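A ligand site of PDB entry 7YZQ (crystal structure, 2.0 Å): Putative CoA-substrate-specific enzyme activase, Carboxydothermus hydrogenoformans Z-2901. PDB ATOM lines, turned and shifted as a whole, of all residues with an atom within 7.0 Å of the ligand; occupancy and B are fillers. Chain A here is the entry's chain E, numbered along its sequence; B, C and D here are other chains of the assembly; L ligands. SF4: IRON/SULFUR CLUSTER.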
ATOM      1  N   LYS A 114     -16.222   6.886 -19.571  1.00  0.00           N
ATOM      2  CA  LYS A 114     -15.215   6.197 -20.376  1.00  0.00           C
ATOM      3  C   LYS A 114     -15.658   6.032 -21.812  1.00  0.00           C
ATOM      4  O   LYS A 114     -14.832   6.128 -22.748  1.00  0.00           O
ATOM      5  CB  LYS A 114     -14.840   4.817 -19.784  1.00  0.00           C
ATOM      6  CG  LYS A 114     -13.883   4.931 -18.591  1.00  0.00           C
ATOM      7  CD  LYS A 114     -13.508   3.579 -17.962  1.00  0.00           C
ATOM      8  CE  LYS A 114     -12.446   2.837 -18.810  1.00  0.00           C
ATOM      9  NZ  LYS A 114     -11.337   3.746 -19.361  1.00  0.00           N
ATOM     10  N   CYS A 115     -16.966   5.829 -22.025  1.00  0.00           N
ATOM     11  CA  CYS A 115     -17.449   5.638 -23.387  1.00  0.00           C
ATOM     12  C   CYS A 115     -17.495   6.938 -24.174  1.00  0.00           C
ATOM     13  O   CYS A 115     -17.610   6.896 -25.400  1.00  0.00           O
ATOM     14  CB  CYS A 115     -18.832   4.999 -23.415  1.00  0.00           C
ATOM     15  SG  CYS A 115     -18.797   3.256 -22.875  1.00  0.00           S
ATOM     16  N   ALA A 116     -17.393   8.088 -23.498  1.00  0.00           N
ATOM     17  CA  ALA A 116     -17.384   9.378 -24.180  1.00  0.00           C
ATOM     18  C   ALA A 116     -15.990   9.949 -24.376  1.00  0.00           C
ATOM     19  O   ALA A 116     -15.856  11.115 -24.750  1.00  0.00           O
ATOM     20  CB  ALA A 116     -18.269  10.386 -23.426  1.00  0.00           C
ATOM     21  N   ALA A 117     -14.946   9.151 -24.157  1.00  0.00           N
ATOM     22  CA  ALA A 117     -13.592   9.618 -24.356  1.00  0.00           C
ATOM     23  C   ALA A 117     -13.290   9.861 -25.816  1.00  0.00           C
ATOM     24  O   ALA A 117     -13.824   9.197 -26.713  1.00  0.00           O
ATOM     25  CB  ALA A 117     -12.588   8.604 -23.789  1.00  0.00           C
ATOM     26  N   MET A 151     -23.273   7.503 -29.085  1.00  0.00           N
ATOM     27  CA  MET A 151     -22.783   6.602 -28.042  1.00  0.00           C
ATOM     28  C   MET A 151     -21.292   6.825 -27.770  1.00  0.00           C
ATOM     29  O   MET A 151     -20.881   7.039 -26.614  1.00  0.00           O
ATOM     30  CB  MET A 151     -23.051   5.157 -28.458  1.00  0.00           C
ATOM     31  CG  MET A 151     -22.604   4.120 -27.463  1.00  0.00           C
ATOM     32  SD  MET A 151     -23.654   4.138 -25.955  1.00  0.00           S
ATOM     33  CE  MET A 151     -22.461   4.586 -24.722  1.00  0.00           C
ATOM     34  N   CYS A 152     -20.487   6.817 -28.822  1.00  0.00           N
ATOM     35  CA  CYS A 152     -19.037   6.865 -28.713  1.00  0.00           C
ATOM     36  C   CYS A 152     -18.485   7.036 -30.114  1.00  0.00           C
ATOM     37  O   CYS A 152     -19.214   6.931 -31.103  1.00  0.00           O
ATOM     38  CB  CYS A 152     -18.497   5.584 -28.070  1.00  0.00           C
ATOM     39  SG  CYS A 152     -18.823   4.141 -29.060  1.00  0.00           S
ATOM     40  N   THR A 153     -17.178   7.239 -30.200  1.00  0.00           N
ATOM     41  CA  THR A 153     -16.553   7.427 -31.502  1.00  0.00           C
ATOM     42  C   THR A 153     -16.467   6.153 -32.314  1.00  0.00           C
ATOM     43  O   THR A 153     -16.383   6.232 -33.547  1.00  0.00           O
ATOM     44  CB  THR A 153     -15.159   8.025 -31.362  1.00  0.00           C
ATOM     45  OG1 THR A 153     -14.282   7.091 -30.728  1.00  0.00           O
ATOM     46  CG2 THR A 153     -15.247   9.290 -30.546  1.00  0.00           C
ATOM     47  N   VAL A 154     -16.446   4.982 -31.676  1.00  0.00           N
ATOM     48  CA  VAL A 154     -16.494   3.743 -32.426  1.00  0.00           C
ATOM     49  C   VAL A 154     -17.822   3.640 -33.174  1.00  0.00           C
ATOM     50  O   VAL A 154     -17.836   3.364 -34.377  1.00  0.00           O
ATOM     51  CB  VAL A 154     -16.266   2.542 -31.504  1.00  0.00           C
ATOM     52  CG1 VAL A 154     -16.613   1.223 -32.227  1.00  0.00           C
ATOM     53  CG2 VAL A 154     -14.854   2.528 -30.976  1.00  0.00           C
ATOM     54  N   PHE A 155     -18.946   3.789 -32.462  1.00  0.00           N
ATOM     55  CA  PHE A 155     -20.243   3.687 -33.119  1.00  0.00           C
ATOM     56  C   PHE A 155     -20.382   4.772 -34.181  1.00  0.00           C
ATOM     57  O   PHE A 155     -20.930   4.525 -35.274  1.00  0.00           O
ATOM     58  CB  PHE A 155     -21.376   3.780 -32.107  1.00  0.00           C
ATOM     59  CG  PHE A 155     -21.528   2.538 -31.237  1.00  0.00           C
ATOM     60  CD1 PHE A 155     -20.491   1.655 -31.112  1.00  0.00           C
ATOM     61  CD2 PHE A 155     -22.695   2.292 -30.554  1.00  0.00           C
ATOM     62  CE1 PHE A 155     -20.649   0.503 -30.293  1.00  0.00           C
ATOM     63  CE2 PHE A 155     -22.836   1.187 -29.771  1.00  0.00           C
ATOM     64  CZ  PHE A 155     -21.809   0.308 -29.643  1.00  0.00           C
ATOM     65  N   LYS B 114     -20.224  -4.625 -32.274  1.00  0.00           N
ATOM     66  CA  LYS B 114     -20.118  -3.176 -32.478  1.00  0.00           C
ATOM     67  C   LYS B 114     -18.949  -2.575 -31.714  1.00  0.00           C
ATOM     68  O   LYS B 114     -18.244  -1.690 -32.243  1.00  0.00           O
ATOM     69  CB  LYS B 114     -21.435  -2.501 -32.078  1.00  0.00           C
ATOM     70  CG  LYS B 114     -22.531  -2.564 -33.177  1.00  0.00           C
ATOM     71  CD  LYS B 114     -23.846  -1.943 -32.748  1.00  0.00           C
ATOM     72  CE  LYS B 114     -23.845  -0.440 -32.957  1.00  0.00           C
ATOM     73  NZ  LYS B 114     -23.230   0.038 -34.239  1.00  0.00           N
ATOM     74  N   CYS B 115     -18.706  -3.040 -30.487  1.00  0.00           N
ATOM     75  CA  CYS B 115     -17.624  -2.454 -29.701  1.00  0.00           C
ATOM     76  C   CYS B 115     -16.240  -2.860 -30.190  1.00  0.00           C
ATOM     77  O   CYS B 115     -15.236  -2.258 -29.755  1.00  0.00           O
ATOM     78  CB  CYS B 115     -17.737  -2.826 -28.238  1.00  0.00           C
ATOM     79  SG  CYS B 115     -19.196  -2.243 -27.464  1.00  0.00           S
ATOM     80  N   ALA B 116     -16.178  -3.860 -31.075  1.00  0.00           N
ATOM     81  CA  ALA B 116     -14.924  -4.309 -31.673  1.00  0.00           C
ATOM     82  C   ALA B 116     -14.689  -3.713 -33.051  1.00  0.00           C
ATOM     83  O   ALA B 116     -13.745  -4.133 -33.736  1.00  0.00           O
ATOM     84  CB  ALA B 116     -14.896  -5.827 -31.762  1.00  0.00           C
ATOM     85  N   ALA B 117     -15.485  -2.721 -33.441  1.00  0.00           N
ATOM     86  CA  ALA B 117     -15.320  -2.111 -34.745  1.00  0.00           C
ATOM     87  C   ALA B 117     -14.092  -1.215 -34.793  1.00  0.00           C
ATOM     88  O   ALA B 117     -13.668  -0.646 -33.788  1.00  0.00           O
ATOM     89  CB  ALA B 117     -16.542  -1.304 -35.105  1.00  0.00           C
ATOM     90  N   MET B 151     -11.236  -4.045 -24.717  1.00  0.00           N
ATOM     91  CA  MET B 151     -12.643  -3.748 -24.908  1.00  0.00           C
ATOM     92  C   MET B 151     -12.938  -3.144 -26.274  1.00  0.00           C
ATOM     93  O   MET B 151     -13.821  -3.610 -26.997  1.00  0.00           O
ATOM     94  CB  MET B 151     -13.120  -2.804 -23.800  1.00  0.00           C
ATOM     95  CG  MET B 151     -14.561  -2.460 -23.876  1.00  0.00           C
ATOM     96  SD  MET B 151     -15.577  -3.913 -23.422  1.00  0.00           S
ATOM     97  CE  MET B 151     -15.534  -3.918 -21.662  1.00  0.00           C
ATOM     98  N   CYS B 152     -12.262  -2.049 -26.619  1.00  0.00           N
ATOM     99  CA  CYS B 152     -12.574  -1.286 -27.813  1.00  0.00           C
ATOM    100  C   CYS B 152     -11.446  -0.295 -27.997  1.00  0.00           C
ATOM    101  O   CYS B 152     -10.588  -0.125 -27.125  1.00  0.00           O
ATOM    102  CB  CYS B 152     -13.917  -0.574 -27.668  1.00  0.00           C
ATOM    103  SG  CYS B 152     -13.843   0.647 -26.322  1.00  0.00           S
ATOM    104  N   THR B 153     -11.486   0.392 -29.128  1.00  0.00           N
ATOM    105  CA  THR B 153     -10.429   1.347 -29.452  1.00  0.00           C
ATOM    106  C   THR B 153     -10.557   2.652 -28.665  1.00  0.00           C
ATOM    107  O   THR B 153      -9.547   3.357 -28.522  1.00  0.00           O
ATOM    108  CB  THR B 153     -10.390   1.681 -30.960  1.00  0.00           C
ATOM    109  OG1 THR B 153     -11.607   2.319 -31.322  1.00  0.00           O
ATOM    110  CG2 THR B 153     -10.191   0.461 -31.797  1.00  0.00           C
ATOM    111  N   VAL B 154     -11.745   2.978 -28.136  1.00  0.00           N
ATOM    112  CA  VAL B 154     -11.888   4.142 -27.271  1.00  0.00           C
ATOM    113  C   VAL B 154     -11.105   3.935 -25.980  1.00  0.00           C
ATOM    114  O   VAL B 154     -10.320   4.793 -25.577  1.00  0.00           O
ATOM    115  CB  VAL B 154     -13.364   4.407 -26.968  1.00  0.00           C
ATOM    116  CG1 VAL B 154     -13.495   5.495 -25.920  1.00  0.00           C
ATOM    117  CG2 VAL B 154     -14.087   4.839 -28.226  1.00  0.00           C
ATOM    118  N   PHE B 155     -11.340   2.793 -25.302  1.00  0.00           N
ATOM    119  CA  PHE B 155     -10.634   2.506 -24.052  1.00  0.00           C
ATOM    120  C   PHE B 155      -9.133   2.316 -24.300  1.00  0.00           C
ATOM    121  O   PHE B 155      -8.303   2.626 -23.429  1.00  0.00           O
ATOM    122  CB  PHE B 155     -11.201   1.254 -23.379  1.00  0.00           C
ATOM    123  CG  PHE B 155     -12.600   1.372 -22.818  1.00  0.00           C
ATOM    124  CD1 PHE B 155     -13.460   2.322 -23.256  1.00  0.00           C
ATOM    125  CD2 PHE B 155     -13.022   0.482 -21.841  1.00  0.00           C
ATOM    126  CE1 PHE B 155     -14.764   2.416 -22.754  1.00  0.00           C
ATOM    127  CE2 PHE B 155     -14.297   0.544 -21.318  1.00  0.00           C
ATOM    128  CZ  PHE B 155     -15.190   1.522 -21.785  1.00  0.00           C
ATOM    129  N   ARG C 111     -25.328   5.679 -19.960  1.00  0.00           N
ATOM    130  CA  ARG C 111     -25.423   5.637 -21.426  1.00  0.00           C
ATOM    131  C   ARG C 111     -25.216   4.218 -21.955  1.00  0.00           C
ATOM    132  O   ARG C 111     -25.779   3.828 -23.003  1.00  0.00           O
ATOM    133  CB  ARG C 111     -24.412   6.624 -22.051  1.00  0.00           C
ATOM    134  CG  ARG C 111     -24.642   8.103 -21.624  1.00  0.00           C
ATOM    135  CD  ARG C 111     -23.767   9.113 -22.414  1.00  0.00           C
ATOM    136  NE  ARG C 111     -22.408   8.600 -22.531  1.00  0.00           N
ATOM    137  CZ  ARG C 111     -21.806   8.386 -23.694  1.00  0.00           C
ATOM    138  NH1 ARG C 111     -20.580   7.886 -23.720  1.00  0.00           N
ATOM    139  NH2 ARG C 111     -22.459   8.663 -24.840  1.00  0.00           N
ATOM    140  N   ASN C 112     -24.442   3.421 -21.241  1.00  0.00           N
ATOM    141  CA  ASN C 112     -24.261   2.021 -21.637  1.00  0.00           C
ATOM    142  C   ASN C 112     -25.302   1.175 -20.886  1.00  0.00           C
ATOM    143  O   ASN C 112     -24.999   0.346 -20.046  1.00  0.00           O
ATOM    144  CB  ASN C 112     -22.814   1.569 -21.424  1.00  0.00           C
ATOM    145  CG  ASN C 112     -22.275   1.954 -20.074  1.00  0.00           C
ATOM    146  OD1 ASN C 112     -22.827   2.857 -19.345  1.00  0.00           O
ATOM    147  ND2 ASN C 112     -21.188   1.284 -19.699  1.00  0.00           N
ATOM    148  N   GLN C 372     -28.291  -3.779 -27.860  1.00  0.00           N
ATOM    149  CA  GLN C 372     -27.040  -3.449 -27.190  1.00  0.00           C
ATOM    150  C   GLN C 372     -27.254  -3.272 -25.697  1.00  0.00           C
ATOM    151  O   GLN C 372     -28.206  -2.622 -25.250  1.00  0.00           O
ATOM    152  CB  GLN C 372     -26.458  -2.162 -27.824  1.00  0.00           C
ATOM    153  CG  GLN C 372     -24.984  -1.847 -27.507  1.00  0.00           C
ATOM    154  CD  GLN C 372     -24.002  -2.689 -28.317  1.00  0.00           C
ATOM    155  OE1 GLN C 372     -24.250  -3.071 -29.468  1.00  0.00           O
ATOM    156  NE2 GLN C 372     -22.868  -2.955 -27.711  1.00  0.00           N
ATOM    157  N   PHE C 373     -26.394  -3.908 -24.904  1.00  0.00           N
ATOM    158  CA  PHE C 373     -26.403  -3.837 -23.447  1.00  0.00           C
ATOM    159  C   PHE C 373     -27.567  -4.594 -22.831  1.00  0.00           C
ATOM    160  O   PHE C 373     -27.785  -4.522 -21.599  1.00  0.00           O
ATOM    161  CB  PHE C 373     -26.384  -2.376 -22.991  1.00  0.00           C
ATOM    162  CG  PHE C 373     -25.302  -1.563 -23.646  1.00  0.00           C
ATOM    163  CD1 PHE C 373     -23.992  -1.931 -23.536  1.00  0.00           C
ATOM    164  CD2 PHE C 373     -25.592  -0.422 -24.357  1.00  0.00           C
ATOM    165  CE1 PHE C 373     -22.987  -1.206 -24.126  1.00  0.00           C
ATOM    166  CE2 PHE C 373     -24.596   0.345 -24.956  1.00  0.00           C
ATOM    167  CZ  PHE C 373     -23.287  -0.066 -24.867  1.00  0.00           C
ATOM    168  N   ARG D 111     -18.793  -9.154 -24.220  1.00  0.00           N
ATOM    169  CA  ARG D 111     -17.718  -8.273 -23.775  1.00  0.00           C
ATOM    170  C   ARG D 111     -18.266  -7.077 -22.988  1.00  0.00           C
ATOM    171  O   ARG D 111     -17.570  -6.574 -22.098  1.00  0.00           O
ATOM    172  CB  ARG D 111     -16.875  -7.854 -24.980  1.00  0.00           C
ATOM    173  CG  ARG D 111     -16.380  -9.082 -25.790  1.00  0.00           C
ATOM    174  CD  ARG D 111     -15.313  -8.800 -26.843  1.00  0.00           C
ATOM    175  NE  ARG D 111     -15.756  -7.711 -27.720  1.00  0.00           N
ATOM    176  CZ  ARG D 111     -15.142  -6.545 -27.761  1.00  0.00           C
ATOM    177  NH1 ARG D 111     -15.601  -5.578 -28.518  1.00  0.00           N
ATOM    178  NH2 ARG D 111     -14.006  -6.369 -27.066  1.00  0.00           N
ATOM    179  N   ASN D 112     -19.507  -6.653 -23.288  1.00  0.00           N
ATOM    180  CA  ASN D 112     -20.231  -5.639 -22.494  1.00  0.00           C
ATOM    181  C   ASN D 112     -20.806  -6.257 -21.205  1.00  0.00           C
ATOM    182  O   ASN D 112     -22.014  -6.296 -21.002  1.00  0.00           O
ATOM    183  CB  ASN D 112     -21.414  -5.046 -23.237  1.00  0.00           C
ATOM    184  CG  ASN D 112     -21.056  -4.343 -24.466  1.00  0.00           C
ATOM    185  OD1 ASN D 112     -21.847  -4.335 -25.431  1.00  0.00           O
ATOM    186  ND2 ASN D 112     -19.884  -3.762 -24.471  1.00  0.00           N
ATOM    187  N   GLN D 372     -17.402  -1.074 -14.642  1.00  0.00           N
ATOM    188  CA  GLN D 372     -18.043  -0.943 -15.961  1.00  0.00           C
ATOM    189  C   GLN D 372     -19.008  -2.076 -16.266  1.00  0.00           C
ATOM    190  O   GLN D 372     -18.681  -3.256 -16.101  1.00  0.00           O
ATOM    191  CB  GLN D 372     -16.937  -0.877 -17.027  1.00  0.00           C
ATOM    192  CG  GLN D 372     -17.390  -0.375 -18.423  1.00  0.00           C
ATOM    193  CD  GLN D 372     -17.518   1.130 -18.515  1.00  0.00           C
ATOM    194  OE1 GLN D 372     -16.994   1.881 -17.678  1.00  0.00           O
ATOM    195  NE2 GLN D 372     -18.202   1.593 -19.560  1.00  0.00           N
ATOM    196  N   PHE D 373     -20.221  -1.695 -16.701  1.00  0.00           N
ATOM    197  CA  PHE D 373     -21.348  -2.550 -17.062  1.00  0.00           C
ATOM    198  C   PHE D 373     -21.991  -3.221 -15.851  1.00  0.00           C
ATOM    199  O   PHE D 373     -22.775  -4.177 -16.046  1.00  0.00           O
ATOM    200  CB  PHE D 373     -20.958  -3.611 -18.100  1.00  0.00           C
ATOM    201  CG  PHE D 373     -20.366  -3.035 -19.324  1.00  0.00           C
ATOM    202  CD1 PHE D 373     -21.147  -2.260 -20.166  1.00  0.00           C
ATOM    203  CD2 PHE D 373     -19.046  -3.218 -19.618  1.00  0.00           C
ATOM    204  CE1 PHE D 373     -20.591  -1.664 -21.288  1.00  0.00           C
ATOM    205  CE2 PHE D 373     -18.509  -2.633 -20.751  1.00  0.00           C
ATOM    206  CZ  PHE D 373     -19.283  -1.843 -21.555  1.00  0.00           C
HETATM  207 FE1  SF4 L   1     -18.506  -0.057 -26.633  1.00  0.00          FE
HETATM  208 FE2  SF4 L   1     -18.218   2.472 -27.503  1.00  0.00          FE
HETATM  209 FE3  SF4 L   1     -16.143   1.172 -26.259  1.00  0.00          FE
HETATM  210 FE4  SF4 L   1     -18.291   2.024 -24.842  1.00  0.00          FE
HETATM  211  S1  SF4 L   1     -16.800   3.334 -25.986  1.00  0.00           S
HETATM  212  S2  SF4 L   1     -17.297  -0.001 -24.695  1.00  0.00           S
HETATM  213  S3  SF4 L   1     -19.953   1.655 -26.325  1.00  0.00           S
HETATM  214  S4  SF4 L   1     -17.083   0.653 -28.255  1.00  0.00           S
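An iron atom (FE3) of the ligand is bound by the side-chain sulfur (SG) of Cys 152 of chain B (2.4 Å).
The side-chain sulfur of Cys 152 of chain A binds an iron atom (FE2) of the ligand (2.4 Å).
The side-chain sulfur (SG) of Cys 115 of chain A is bound to an iron atom (FE4) of the ligand (2.4 Å).
The side-chain sulfur (SG) of Cys 115 of chain B binds an iron atom (FE1) of the ligand, at 2.4 Å.
The backbone NH of Val 154 of chain B lies close to the side-chain sulfur of Cys 152 of chain B, 3.6 Å away.
The backbone NH (N) of Val 154 of chain A sits close to the side-chain sulfur (SG) of Cys 152 of chain A, at 3.6 Å.
The backbone NH (N) of Phe 155 of chain A sits close to the side-chain sulfur (SG) of Cys 152 of chain A.
NE2 of Gln 372 of chain D lies close to SG of Cys 115 of chain A, 3.8 Å away.
The side-chain sulfur of Cys 115 of chain B sits close to the side-chain amide nitrogen of Asn 112 of chain D (3.4 Å).
The side-chain sulfur of Cys 115 of chain B sits close to the side-chain amide nitrogen of Gln 372 of chain C, 3.7 Å away.
O of Met 151 of chain B is in hydrogen-bond range of NH2 of Arg 111 of chain D, 2.8 Å away.
The guanidinium group of Arg 111 of chain C is in hydrogen-bond range of the backbone carbonyl oxygen of Met 151 of chain A (2.9 Å).
Met 151 of chain A touches the ligand.
CB of Val 154 of chain A touches S4 of the ligand, at 3.8 Å.
Met 151 of chain B touches the ligand.
Val 154 of chain B touches the ligand.
Phe 155 of chain B touches the ligand (CZ to S2, 3.9 Å).
Hydrophobic or aromatic side chains that line the ligand: Met 151 of chain A, Val 154 of chain A, Met 151 of chain B, Val 154 of chain B and Phe 155 of chain B.
Of the 26 residues printed, 9 come within 4 Å of the ligand.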
